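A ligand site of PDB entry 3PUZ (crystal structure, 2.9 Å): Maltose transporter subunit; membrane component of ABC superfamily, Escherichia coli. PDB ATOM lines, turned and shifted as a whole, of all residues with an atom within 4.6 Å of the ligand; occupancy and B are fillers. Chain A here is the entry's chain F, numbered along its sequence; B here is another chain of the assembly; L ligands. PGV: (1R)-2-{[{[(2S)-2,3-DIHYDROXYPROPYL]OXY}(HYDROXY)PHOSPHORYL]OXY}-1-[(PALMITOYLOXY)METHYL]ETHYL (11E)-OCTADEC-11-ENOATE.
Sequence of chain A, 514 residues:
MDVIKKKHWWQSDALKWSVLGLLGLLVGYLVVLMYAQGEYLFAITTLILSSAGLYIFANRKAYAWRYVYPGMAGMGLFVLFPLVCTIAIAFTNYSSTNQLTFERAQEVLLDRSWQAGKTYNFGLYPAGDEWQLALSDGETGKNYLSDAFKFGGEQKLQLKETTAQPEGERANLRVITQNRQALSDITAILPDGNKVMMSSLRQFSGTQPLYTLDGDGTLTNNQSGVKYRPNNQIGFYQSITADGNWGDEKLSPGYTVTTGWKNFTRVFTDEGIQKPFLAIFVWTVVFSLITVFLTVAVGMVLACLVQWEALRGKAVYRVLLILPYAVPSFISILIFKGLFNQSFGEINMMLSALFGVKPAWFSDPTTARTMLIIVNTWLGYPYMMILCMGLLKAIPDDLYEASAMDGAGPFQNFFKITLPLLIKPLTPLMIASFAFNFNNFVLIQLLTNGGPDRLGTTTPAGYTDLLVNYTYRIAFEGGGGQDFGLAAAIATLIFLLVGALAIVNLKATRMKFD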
ATOM      1  N   PHE A 293      21.012  28.548 -18.657  1.00  0.00           N
ATOM      2  CA  PHE A 293      20.455  28.013 -19.900  1.00  0.00           C
ATOM      3  C   PHE A 293      19.007  27.570 -19.753  1.00  0.00           C
ATOM      4  O   PHE A 293      18.168  27.876 -20.601  1.00  0.00           O
ATOM      5  CB  PHE A 293      21.319  26.865 -20.440  1.00  0.00           C
ATOM      6  CG  PHE A 293      20.719  26.177 -21.639  1.00  0.00           C
ATOM      7  CD1 PHE A 293      20.776  26.762 -22.901  1.00  0.00           C
ATOM      8  CD2 PHE A 293      20.116  24.930 -21.514  1.00  0.00           C
ATOM      9  CE1 PHE A 293      20.222  26.130 -24.024  1.00  0.00           C
ATOM     10  CE2 PHE A 293      19.553  24.284 -22.622  1.00  0.00           C
ATOM     11  CZ  PHE A 293      19.614  24.879 -23.876  1.00  0.00           C
ATOM     12  N   VAL A 296      16.563  30.628 -18.664  1.00  0.00           N
ATOM     13  CA  VAL A 296      16.309  31.480 -19.831  1.00  0.00           C
ATOM     14  C   VAL A 296      15.339  30.789 -20.797  1.00  0.00           C
ATOM     15  O   VAL A 296      14.382  31.397 -21.256  1.00  0.00           O
ATOM     16  CB  VAL A 296      17.605  31.880 -20.582  1.00  0.00           C
ATOM     17  CG1 VAL A 296      17.295  32.464 -21.953  1.00  0.00           C
ATOM     18  CG2 VAL A 296      18.398  32.887 -19.779  1.00  0.00           C
ATOM     19  N   ALA A 297      15.602  29.513 -21.091  1.00  0.00           N
ATOM     20  CA  ALA A 297      14.746  28.733 -21.975  1.00  0.00           C
ATOM     21  C   ALA A 297      13.298  28.734 -21.493  1.00  0.00           C
ATOM     22  O   ALA A 297      12.408  29.207 -22.199  1.00  0.00           O
ATOM     23  CB  ALA A 297      15.269  27.312 -22.127  1.00  0.00           C
ATOM     24  N   VAL A 298      13.089  28.239 -20.271  1.00  0.00           N
ATOM     25  CA  VAL A 298      11.758  28.187 -19.664  1.00  0.00           C
ATOM     26  C   VAL A 298      11.148  29.593 -19.526  1.00  0.00           C
ATOM     27  O   VAL A 298       9.977  29.797 -19.836  1.00  0.00           O
ATOM     28  CB  VAL A 298      11.779  27.473 -18.288  1.00  0.00           C
ATOM     29  CG1 VAL A 298      10.404  27.497 -17.628  1.00  0.00           C
ATOM     30  CG2 VAL A 298      12.255  26.028 -18.452  1.00  0.00           C
ATOM     31  N   VAL A 301      10.254  31.045 -23.258  1.00  0.00           N
ATOM     32  CA  VAL A 301       9.187  30.300 -23.915  1.00  0.00           C
ATOM     33  C   VAL A 301       7.826  30.631 -23.318  1.00  0.00           C
ATOM     34  O   VAL A 301       6.848  30.789 -24.049  1.00  0.00           O
ATOM     35  CB  VAL A 301       9.453  28.761 -23.879  1.00  0.00           C
ATOM     36  CG1 VAL A 301       8.253  27.987 -24.409  1.00  0.00           C
ATOM     37  CG2 VAL A 301      10.682  28.417 -24.695  1.00  0.00           C
ATOM     38  N   LEU A 302       7.772  30.756 -21.992  1.00  0.00           N
ATOM     39  CA  LEU A 302       6.540  31.111 -21.303  1.00  0.00           C
ATOM     40  C   LEU A 302       6.168  32.590 -21.505  1.00  0.00           C
ATOM     41  O   LEU A 302       4.988  32.908 -21.690  1.00  0.00           O
ATOM     42  CB  LEU A 302       6.634  30.785 -19.807  1.00  0.00           C
ATOM     43  CG  LEU A 302       6.429  29.318 -19.399  1.00  0.00           C
ATOM     44  CD1 LEU A 302       7.038  29.071 -18.038  1.00  0.00           C
ATOM     45  CD2 LEU A 302       4.966  28.919 -19.418  1.00  0.00           C
ATOM     46  N   CYS A 304       6.766  34.328 -24.057  1.00  0.00           N
ATOM     47  CA  CYS A 304       6.206  34.397 -25.402  1.00  0.00           C
ATOM     48  C   CYS A 304       4.752  33.909 -25.419  1.00  0.00           C
ATOM     49  O   CYS A 304       3.915  34.457 -26.127  1.00  0.00           O
ATOM     50  CB  CYS A 304       7.034  33.558 -26.378  1.00  0.00           C
ATOM     51  SG  CYS A 304       8.689  34.196 -26.711  1.00  0.00           S
ATOM     52  N   LEU A 305       4.477  32.874 -24.617  1.00  0.00           N
ATOM     53  CA  LEU A 305       3.163  32.230 -24.607  1.00  0.00           C
ATOM     54  C   LEU A 305       2.103  33.020 -23.847  1.00  0.00           C
ATOM     55  O   LEU A 305       0.938  33.029 -24.239  1.00  0.00           O
ATOM     56  CB  LEU A 305       3.265  30.810 -24.047  1.00  0.00           C
ATOM     57  CG  LEU A 305       3.808  29.745 -25.013  1.00  0.00           C
ATOM     58  CD1 LEU A 305       4.110  28.453 -24.278  1.00  0.00           C
ATOM     59  CD2 LEU A 305       2.848  29.499 -26.152  1.00  0.00           C
ATOM     60  N   GLN A 307       1.999  36.294 -23.502  1.00  0.00           N
ATOM     61  CA  GLN A 307       1.640  37.471 -24.296  1.00  0.00           C
ATOM     62  C   GLN A 307       1.014  37.122 -25.649  1.00  0.00           C
ATOM     63  O   GLN A 307       0.580  38.004 -26.381  1.00  0.00           O
ATOM     64  CB  GLN A 307       2.853  38.399 -24.473  1.00  0.00           C
ATOM     65  CG  GLN A 307       3.824  37.986 -25.582  1.00  0.00           C
ATOM     66  CD  GLN A 307       4.560  39.174 -26.173  1.00  0.00           C
ATOM     67  OE1 GLN A 307       5.040  40.050 -25.457  1.00  0.00           O
ATOM     68  NE2 GLN A 307       4.653  39.204 -27.503  1.00  0.00           N
ATOM     69  N   TRP A 308       0.962  35.830 -25.969  1.00  0.00           N
ATOM     70  CA  TRP A 308       0.385  35.339 -27.223  1.00  0.00           C
ATOM     71  C   TRP A 308      -1.106  35.672 -27.317  1.00  0.00           C
ATOM     72  O   TRP A 308      -1.908  35.252 -26.476  1.00  0.00           O
ATOM     73  CB  TRP A 308       0.635  33.836 -27.383  1.00  0.00           C
ATOM     74  CG  TRP A 308       0.046  33.203 -28.618  1.00  0.00           C
ATOM     75  CD1 TRP A 308      -0.138  33.794 -29.841  1.00  0.00           C
ATOM     76  CD2 TRP A 308      -0.403  31.847 -28.760  1.00  0.00           C
ATOM     77  NE1 TRP A 308      -0.691  32.898 -30.726  1.00  0.00           N
ATOM     78  CE2 TRP A 308      -0.858  31.692 -30.089  1.00  0.00           C
ATOM     79  CE3 TRP A 308      -0.456  30.749 -27.898  1.00  0.00           C
ATOM     80  CZ2 TRP A 308      -1.371  30.488 -30.570  1.00  0.00           C
ATOM     81  CZ3 TRP A 308      -0.969  29.547 -28.369  1.00  0.00           C
ATOM     82  CH2 TRP A 308      -1.417  29.425 -29.698  1.00  0.00           C
ATOM     83  N   TYR A 400       6.537  40.490 -37.171  1.00  0.00           N
ATOM     84  CA  TYR A 400       5.826  39.220 -37.211  1.00  0.00           C
ATOM     85  C   TYR A 400       4.737  39.234 -38.282  1.00  0.00           C
ATOM     86  O   TYR A 400       4.295  38.184 -38.745  1.00  0.00           O
ATOM     87  CB  TYR A 400       5.221  38.889 -35.842  1.00  0.00           C
ATOM     88  CG  TYR A 400       6.253  38.649 -34.759  1.00  0.00           C
ATOM     89  CD1 TYR A 400       6.321  39.497 -33.655  1.00  0.00           C
ATOM     90  CD2 TYR A 400       7.146  37.588 -34.826  1.00  0.00           C
ATOM     91  CE1 TYR A 400       7.263  39.285 -32.649  1.00  0.00           C
ATOM     92  CE2 TYR A 400       8.097  37.369 -33.829  1.00  0.00           C
ATOM     93  CZ  TYR A 400       8.146  38.221 -32.746  1.00  0.00           C
ATOM     94  OH  TYR A 400       9.074  38.004 -31.749  1.00  0.00           O
ATOM     95  N   GLY A 409       5.666  29.749 -39.589  1.00  0.00           N
ATOM     96  CA  GLY A 409       4.929  29.144 -38.482  1.00  0.00           C
ATOM     97  C   GLY A 409       5.434  29.666 -37.141  1.00  0.00           C
ATOM     98  O   GLY A 409       6.452  30.368 -37.092  1.00  0.00           O
ATOM     99  N   PRO A 410       4.715  29.344 -36.049  1.00  0.00           N
ATOM    100  CA  PRO A 410       5.097  29.750 -34.692  1.00  0.00           C
ATOM    101  C   PRO A 410       6.540  29.401 -34.342  1.00  0.00           C
ATOM    102  O   PRO A 410       7.251  30.233 -33.768  1.00  0.00           O
ATOM    103  CB  PRO A 410       4.116  28.967 -33.817  1.00  0.00           C
ATOM    104  CG  PRO A 410       2.902  28.858 -34.662  1.00  0.00           C
ATOM    105  CD  PRO A 410       3.424  28.634 -36.053  1.00  0.00           C
ATOM    106  N   PHE A 411       6.961  28.179 -34.669  1.00  0.00           N
ATOM    107  CA  PHE A 411       8.337  27.730 -34.424  1.00  0.00           C
ATOM    108  C   PHE A 411       9.349  28.542 -35.225  1.00  0.00           C
ATOM    109  O   PHE A 411      10.366  28.985 -34.681  1.00  0.00           O
ATOM    110  CB  PHE A 411       8.494  26.232 -34.748  1.00  0.00           C
ATOM    111  CG  PHE A 411       7.777  25.319 -33.796  1.00  0.00           C
ATOM    112  CD1 PHE A 411       6.589  24.702 -34.172  1.00  0.00           C
ATOM    113  CD2 PHE A 411       8.302  25.066 -32.534  1.00  0.00           C
ATOM    114  CE1 PHE A 411       5.913  23.848 -33.300  1.00  0.00           C
ATOM    115  CE2 PHE A 411       7.636  24.210 -31.652  1.00  0.00           C
ATOM    116  CZ  PHE A 411       6.439  23.598 -32.029  1.00  0.00           C
ATOM    117  N   ASN A 413       8.960  31.581 -36.392  1.00  0.00           N
ATOM    118  CA  ASN A 413       8.986  32.907 -35.769  1.00  0.00           C
ATOM    119  C   ASN A 413       9.925  32.978 -34.581  1.00  0.00           C
ATOM    120  O   ASN A 413      10.678  33.944 -34.439  1.00  0.00           O
ATOM    121  CB  ASN A 413       7.577  33.324 -35.340  1.00  0.00           C
ATOM    122  CG  ASN A 413       6.811  34.052 -36.431  1.00  0.00           C
ATOM    123  OD1 ASN A 413       7.394  34.480 -37.432  1.00  0.00           O
ATOM    124  ND2 ASN A 413       5.517  34.216 -36.228  1.00  0.00           N
ATOM    125  N   PHE A 414       9.881  31.955 -33.730  1.00  0.00           N
ATOM    126  CA  PHE A 414      10.673  31.933 -32.500  1.00  0.00           C
ATOM    127  C   PHE A 414      12.188  31.910 -32.761  1.00  0.00           C
ATOM    128  O   PHE A 414      12.933  32.698 -32.186  1.00  0.00           O
ATOM    129  CB  PHE A 414      10.271  30.744 -31.620  1.00  0.00           C
ATOM    130  CG  PHE A 414      10.958  30.719 -30.282  1.00  0.00           C
ATOM    131  CD1 PHE A 414      12.093  29.946 -30.074  1.00  0.00           C
ATOM    132  CD2 PHE A 414      10.478  31.479 -29.215  1.00  0.00           C
ATOM    133  CE1 PHE A 414      12.737  29.926 -28.839  1.00  0.00           C
ATOM    134  CE2 PHE A 414      11.114  31.465 -27.981  1.00  0.00           C
ATOM    135  CZ  PHE A 414      12.248  30.686 -27.793  1.00  0.00           C
ATOM    136  N   PHE A 415      12.620  30.995 -33.639  1.00  0.00           N
ATOM    137  CA  PHE A 415      14.050  30.765 -33.840  1.00  0.00           C
ATOM    138  C   PHE A 415      14.712  31.742 -34.807  1.00  0.00           C
ATOM    139  O   PHE A 415      15.900  32.039 -34.665  1.00  0.00           O
ATOM    140  CB  PHE A 415      14.318  29.307 -34.252  1.00  0.00           C
ATOM    141  CG  PHE A 415      14.053  28.306 -33.159  1.00  0.00           C
ATOM    142  CD1 PHE A 415      12.951  27.470 -33.219  1.00  0.00           C
ATOM    143  CD2 PHE A 415      14.926  28.193 -32.074  1.00  0.00           C
ATOM    144  CE1 PHE A 415      12.700  26.542 -32.209  1.00  0.00           C
ATOM    145  CE2 PHE A 415      14.689  27.269 -31.065  1.00  0.00           C
ATOM    146  CZ  PHE A 415      13.578  26.439 -31.126  1.00  0.00           C
ATOM    147  N   LEU A 419      14.091  34.730 -30.754  1.00  0.00           N
ATOM    148  CA  LEU A 419      15.291  34.351 -30.013  1.00  0.00           C
ATOM    149  C   LEU A 419      16.516  35.235 -30.313  1.00  0.00           C
ATOM    150  O   LEU A 419      17.047  35.867 -29.397  1.00  0.00           O
ATOM    151  CB  LEU A 419      15.608  32.860 -30.200  1.00  0.00           C
ATOM    152  CG  LEU A 419      16.649  32.182 -29.288  1.00  0.00           C
ATOM    153  CD1 LEU A 419      16.263  30.726 -29.042  1.00  0.00           C
ATOM    154  CD2 LEU A 419      18.064  32.267 -29.866  1.00  0.00           C
ATOM    155  N   ARG B  12      -2.696  23.972 -32.132  1.00  0.00           N
ATOM    156  CA  ARG B  12      -1.598  24.434 -31.285  1.00  0.00           C
ATOM    157  C   ARG B  12      -2.094  25.141 -30.027  1.00  0.00           C
ATOM    158  O   ARG B  12      -1.443  25.094 -28.992  1.00  0.00           O
ATOM    159  CB  ARG B  12      -0.675  25.361 -32.072  1.00  0.00           C
ATOM    160  CG  ARG B  12       0.203  24.649 -33.085  1.00  0.00           C
ATOM    161  CD  ARG B  12       1.141  25.624 -33.762  1.00  0.00           C
ATOM    162  NE  ARG B  12       0.411  26.625 -34.545  1.00  0.00           N
ATOM    163  CZ  ARG B  12       0.085  26.484 -35.821  1.00  0.00           C
ATOM    164  NH1 ARG B  12       0.441  25.388 -36.491  1.00  0.00           N
ATOM    165  NH2 ARG B  12      -0.580  27.448 -36.442  1.00  0.00           N
ATOM    166  N   THR B  16      -1.432  23.827 -26.199  1.00  0.00           N
ATOM    167  CA  THR B  16      -0.708  24.779 -25.356  1.00  0.00           C
ATOM    168  C   THR B  16      -1.408  24.940 -24.003  1.00  0.00           C
ATOM    169  O   THR B  16      -0.751  25.012 -22.960  1.00  0.00           O
ATOM    170  CB  THR B  16      -0.556  26.155 -26.049  1.00  0.00           C
ATOM    171  OG1 THR B  16       0.212  26.000 -27.251  1.00  0.00           O
ATOM    172  CG2 THR B  16       0.137  27.165 -25.149  1.00  0.00           C
ATOM    173  N   LEU B  19      -0.466  21.995 -21.878  1.00  0.00           N
ATOM    174  CA  LEU B  19       0.948  22.041 -21.501  1.00  0.00           C
ATOM    175  C   LEU B  19       1.260  23.026 -20.382  1.00  0.00           C
ATOM    176  O   LEU B  19       2.070  22.737 -19.494  1.00  0.00           O
ATOM    177  CB  LEU B  19       1.830  22.301 -22.727  1.00  0.00           C
ATOM    178  CG  LEU B  19       2.628  21.130 -23.311  1.00  0.00           C
ATOM    179  CD1 LEU B  19       1.853  19.815 -23.305  1.00  0.00           C
ATOM    180  CD2 LEU B  19       3.103  21.468 -24.708  1.00  0.00           C
ATOM    181  N   LEU B  20       0.616  24.188 -20.414  1.00  0.00           N
ATOM    182  CA  LEU B  20       0.712  25.166 -19.336  1.00  0.00           C
ATOM    183  C   LEU B  20      -0.065  24.702 -18.110  1.00  0.00           C
ATOM    184  O   LEU B  20       0.376  24.876 -16.982  1.00  0.00           O
ATOM    185  CB  LEU B  20       0.207  26.542 -19.785  1.00  0.00           C
ATOM    186  CG  LEU B  20       1.231  27.556 -20.320  1.00  0.00           C
ATOM    187  CD1 LEU B  20       1.779  27.135 -21.679  1.00  0.00           C
ATOM    188  CD2 LEU B  20       0.587  28.935 -20.422  1.00  0.00           C
ATOM    189  N   PHE B  23       1.944  22.306 -16.519  1.00  0.00           N
ATOM    190  CA  PHE B  23       3.127  23.004 -16.000  1.00  0.00           C
ATOM    191  C   PHE B  23       2.836  23.740 -14.685  1.00  0.00           C
ATOM    192  O   PHE B  23       3.630  23.661 -13.761  1.00  0.00           O
ATOM    193  CB  PHE B  23       3.689  23.994 -17.039  1.00  0.00           C
ATOM    194  CG  PHE B  23       5.044  24.555 -16.685  1.00  0.00           C
ATOM    195  CD1 PHE B  23       6.200  23.862 -17.009  1.00  0.00           C
ATOM    196  CD2 PHE B  23       5.151  25.781 -16.039  1.00  0.00           C
ATOM    197  CE1 PHE B  23       7.454  24.379 -16.681  1.00  0.00           C
ATOM    198  CE2 PHE B  23       6.404  26.301 -15.701  1.00  0.00           C
ATOM    199  CZ  PHE B  23       7.556  25.597 -16.032  1.00  0.00           C
HETATM  200  P   PGV L   1       3.029  33.406 -33.429  1.00  0.00           P
HETATM  201  C01 PGV L   1       3.468  31.492 -29.407  1.00  0.00           C
HETATM  202  C02 PGV L   1       2.907  30.656 -30.547  1.00  0.00           C
HETATM  203  C03 PGV L   1       2.322  31.570 -31.624  1.00  0.00           C
HETATM  204  C04 PGV L   1       3.623  35.993 -33.276  1.00  0.00           C
HETATM  205  C05 PGV L   1       3.141  36.590 -31.958  1.00  0.00           C
HETATM  206  C06 PGV L   1       3.402  38.095 -31.964  1.00  0.00           C
HETATM  207  O01 PGV L   1       1.873  29.808 -30.036  1.00  0.00           O
HETATM  208  O02 PGV L   1       1.836  27.938 -31.392  1.00  0.00           O
HETATM  209  O03 PGV L   1       4.862  31.696 -29.622  1.00  0.00           O
HETATM  210  O04 PGV L   1       5.923  30.849 -27.752  1.00  0.00           O
HETATM  211  O05 PGV L   1       3.819  35.977 -30.853  1.00  0.00           O
HETATM  212  O06 PGV L   1       3.400  38.610 -30.631  1.00  0.00           O
HETATM  213  O11 PGV L   1       3.325  32.436 -32.180  1.00  0.00           O
HETATM  214  O12 PGV L   1       4.019  34.636 -33.098  1.00  0.00           O
HETATM  215  O13 PGV L   1       1.604  33.887 -33.379  1.00  0.00           O
HETATM  216  O14 PGV L   1       3.526  32.724 -34.683  1.00  0.00           O
HETATM  217  C1  PGV L   1       2.090  28.394 -30.281  1.00  0.00           C
HETATM  218  C2  PGV L   1       2.600  27.496 -29.175  1.00  0.00           C
HETATM  219  C3  PGV L   1       2.977  26.095 -29.668  1.00  0.00           C
HETATM  220  C4  PGV L   1       3.126  25.110 -28.514  1.00  0.00           C
HETATM  221  C5  PGV L   1       4.585  24.774 -28.251  1.00  0.00           C
HETATM  222  C6  PGV L   1       4.762  23.996 -26.947  1.00  0.00           C
HETATM  223  C7  PGV L   1       5.637  24.769 -25.968  1.00  0.00           C
HETATM  224  C8  PGV L   1       5.717  24.075 -24.610  1.00  0.00           C
HETATM  225  C9  PGV L   1       4.871  24.792 -23.558  1.00  0.00           C
HETATM  226  C10 PGV L   1       5.088  24.209 -22.163  1.00  0.00           C
HETATM  227  C11 PGV L   1       5.650  25.261 -21.217  1.00  0.00           C
HETATM  228  C12 PGV L   1       6.914  24.758 -20.528  1.00  0.00           C
HETATM  229  C13 PGV L   1       8.160  25.471 -21.042  1.00  0.00           C
HETATM  230  C14 PGV L   1       9.404  24.632 -20.800  1.00  0.00           C
HETATM  231  C15 PGV L   1      10.238  24.501 -22.074  1.00  0.00           C
HETATM  232  C16 PGV L   1      11.592  23.852 -21.784  1.00  0.00           C
HETATM  233  C17 PGV L   1      12.531  23.971 -22.974  1.00  0.00           C
HETATM  234  C18 PGV L   1      13.887  23.370 -22.677  1.00  0.00           C
HETATM  235  C19 PGV L   1       5.833  30.839 -28.970  1.00  0.00           C
HETATM  236  C20 PGV L   1       6.734  29.953 -29.802  1.00  0.00           C
HETATM  237  C21 PGV L   1       6.667  28.506 -29.300  1.00  0.00           C
HETATM  238  C22 PGV L   1       7.945  28.145 -28.547  1.00  0.00           C
HETATM  239  C23 PGV L   1       8.481  26.792 -29.009  1.00  0.00           C
HETATM  240  C24 PGV L   1       9.995  26.737 -28.898  1.00  0.00           C
HETATM  241  C25 PGV L   1      10.440  25.903 -27.703  1.00  0.00           C
HETATM  242  C26 PGV L   1      11.875  25.416 -27.875  1.00  0.00           C
HETATM  243  C27 PGV L   1      12.738  25.849 -26.700  1.00  0.00           C
HETATM  244  C28 PGV L   1      14.174  25.367 -26.854  1.00  0.00           C
HETATM  245  C29 PGV L   1      15.095  26.502 -27.304  1.00  0.00           C
HETATM  246  C30 PGV L   1      16.074  26.882 -26.201  1.00  0.00           C
HETATM  247  C31 PGV L   1      16.235  28.392 -26.101  1.00  0.00           C
HETATM  248  C32 PGV L   1      17.711  28.782 -26.131  1.00  0.00           C
HETATM  249  C33 PGV L   1      18.009  29.888 -25.117  1.00  0.00           C
HETATM  250  C34 PGV L   1      19.482  30.235 -25.135  1.00  0.00           C
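The side-chain amide nitrogen of Gln 307 lies within hydrogen-bond range of an oxygen (O06) of the ligand, 3.4 Å away. ND2 of Asn 413 sits at hydrogen-bond distance from O14 of the ligand (2.9 Å).
The side-chain hydroxyl (OG1) of Thr 16 of chain B is in hydrogen-bond range of the backbone carbonyl oxygen (O) of Arg 12 of chain B, 2.6 Å away. N of Leu 419 sits at hydrogen-bond distance from O of Phe 414.
Merely in contact with the ligand: Val 298, Val 301, Cys 304, Leu 305, Trp 308, Tyr 400, Pro 410, Phe 411, Phe 415, Leu 419, Arg 12 of chain B, Thr 16 of chain B, Leu 19 of chain B and Phe 23 of chain B. 16 residues have an atom within 4 Å of the ligand: Val 298, Val 301, Cys 304, Leu 305, Gln 307, Trp 308, Tyr 400, Pro 410, Phe 411, Asn 413, Phe 415, Leu 419, Arg 12 of chain B, Thr 16 of chain B, Leu 19 of chain B and Phe 23 of chain B. Along chain A the residues within 4 Å of the ligand span positions 298 to 419.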
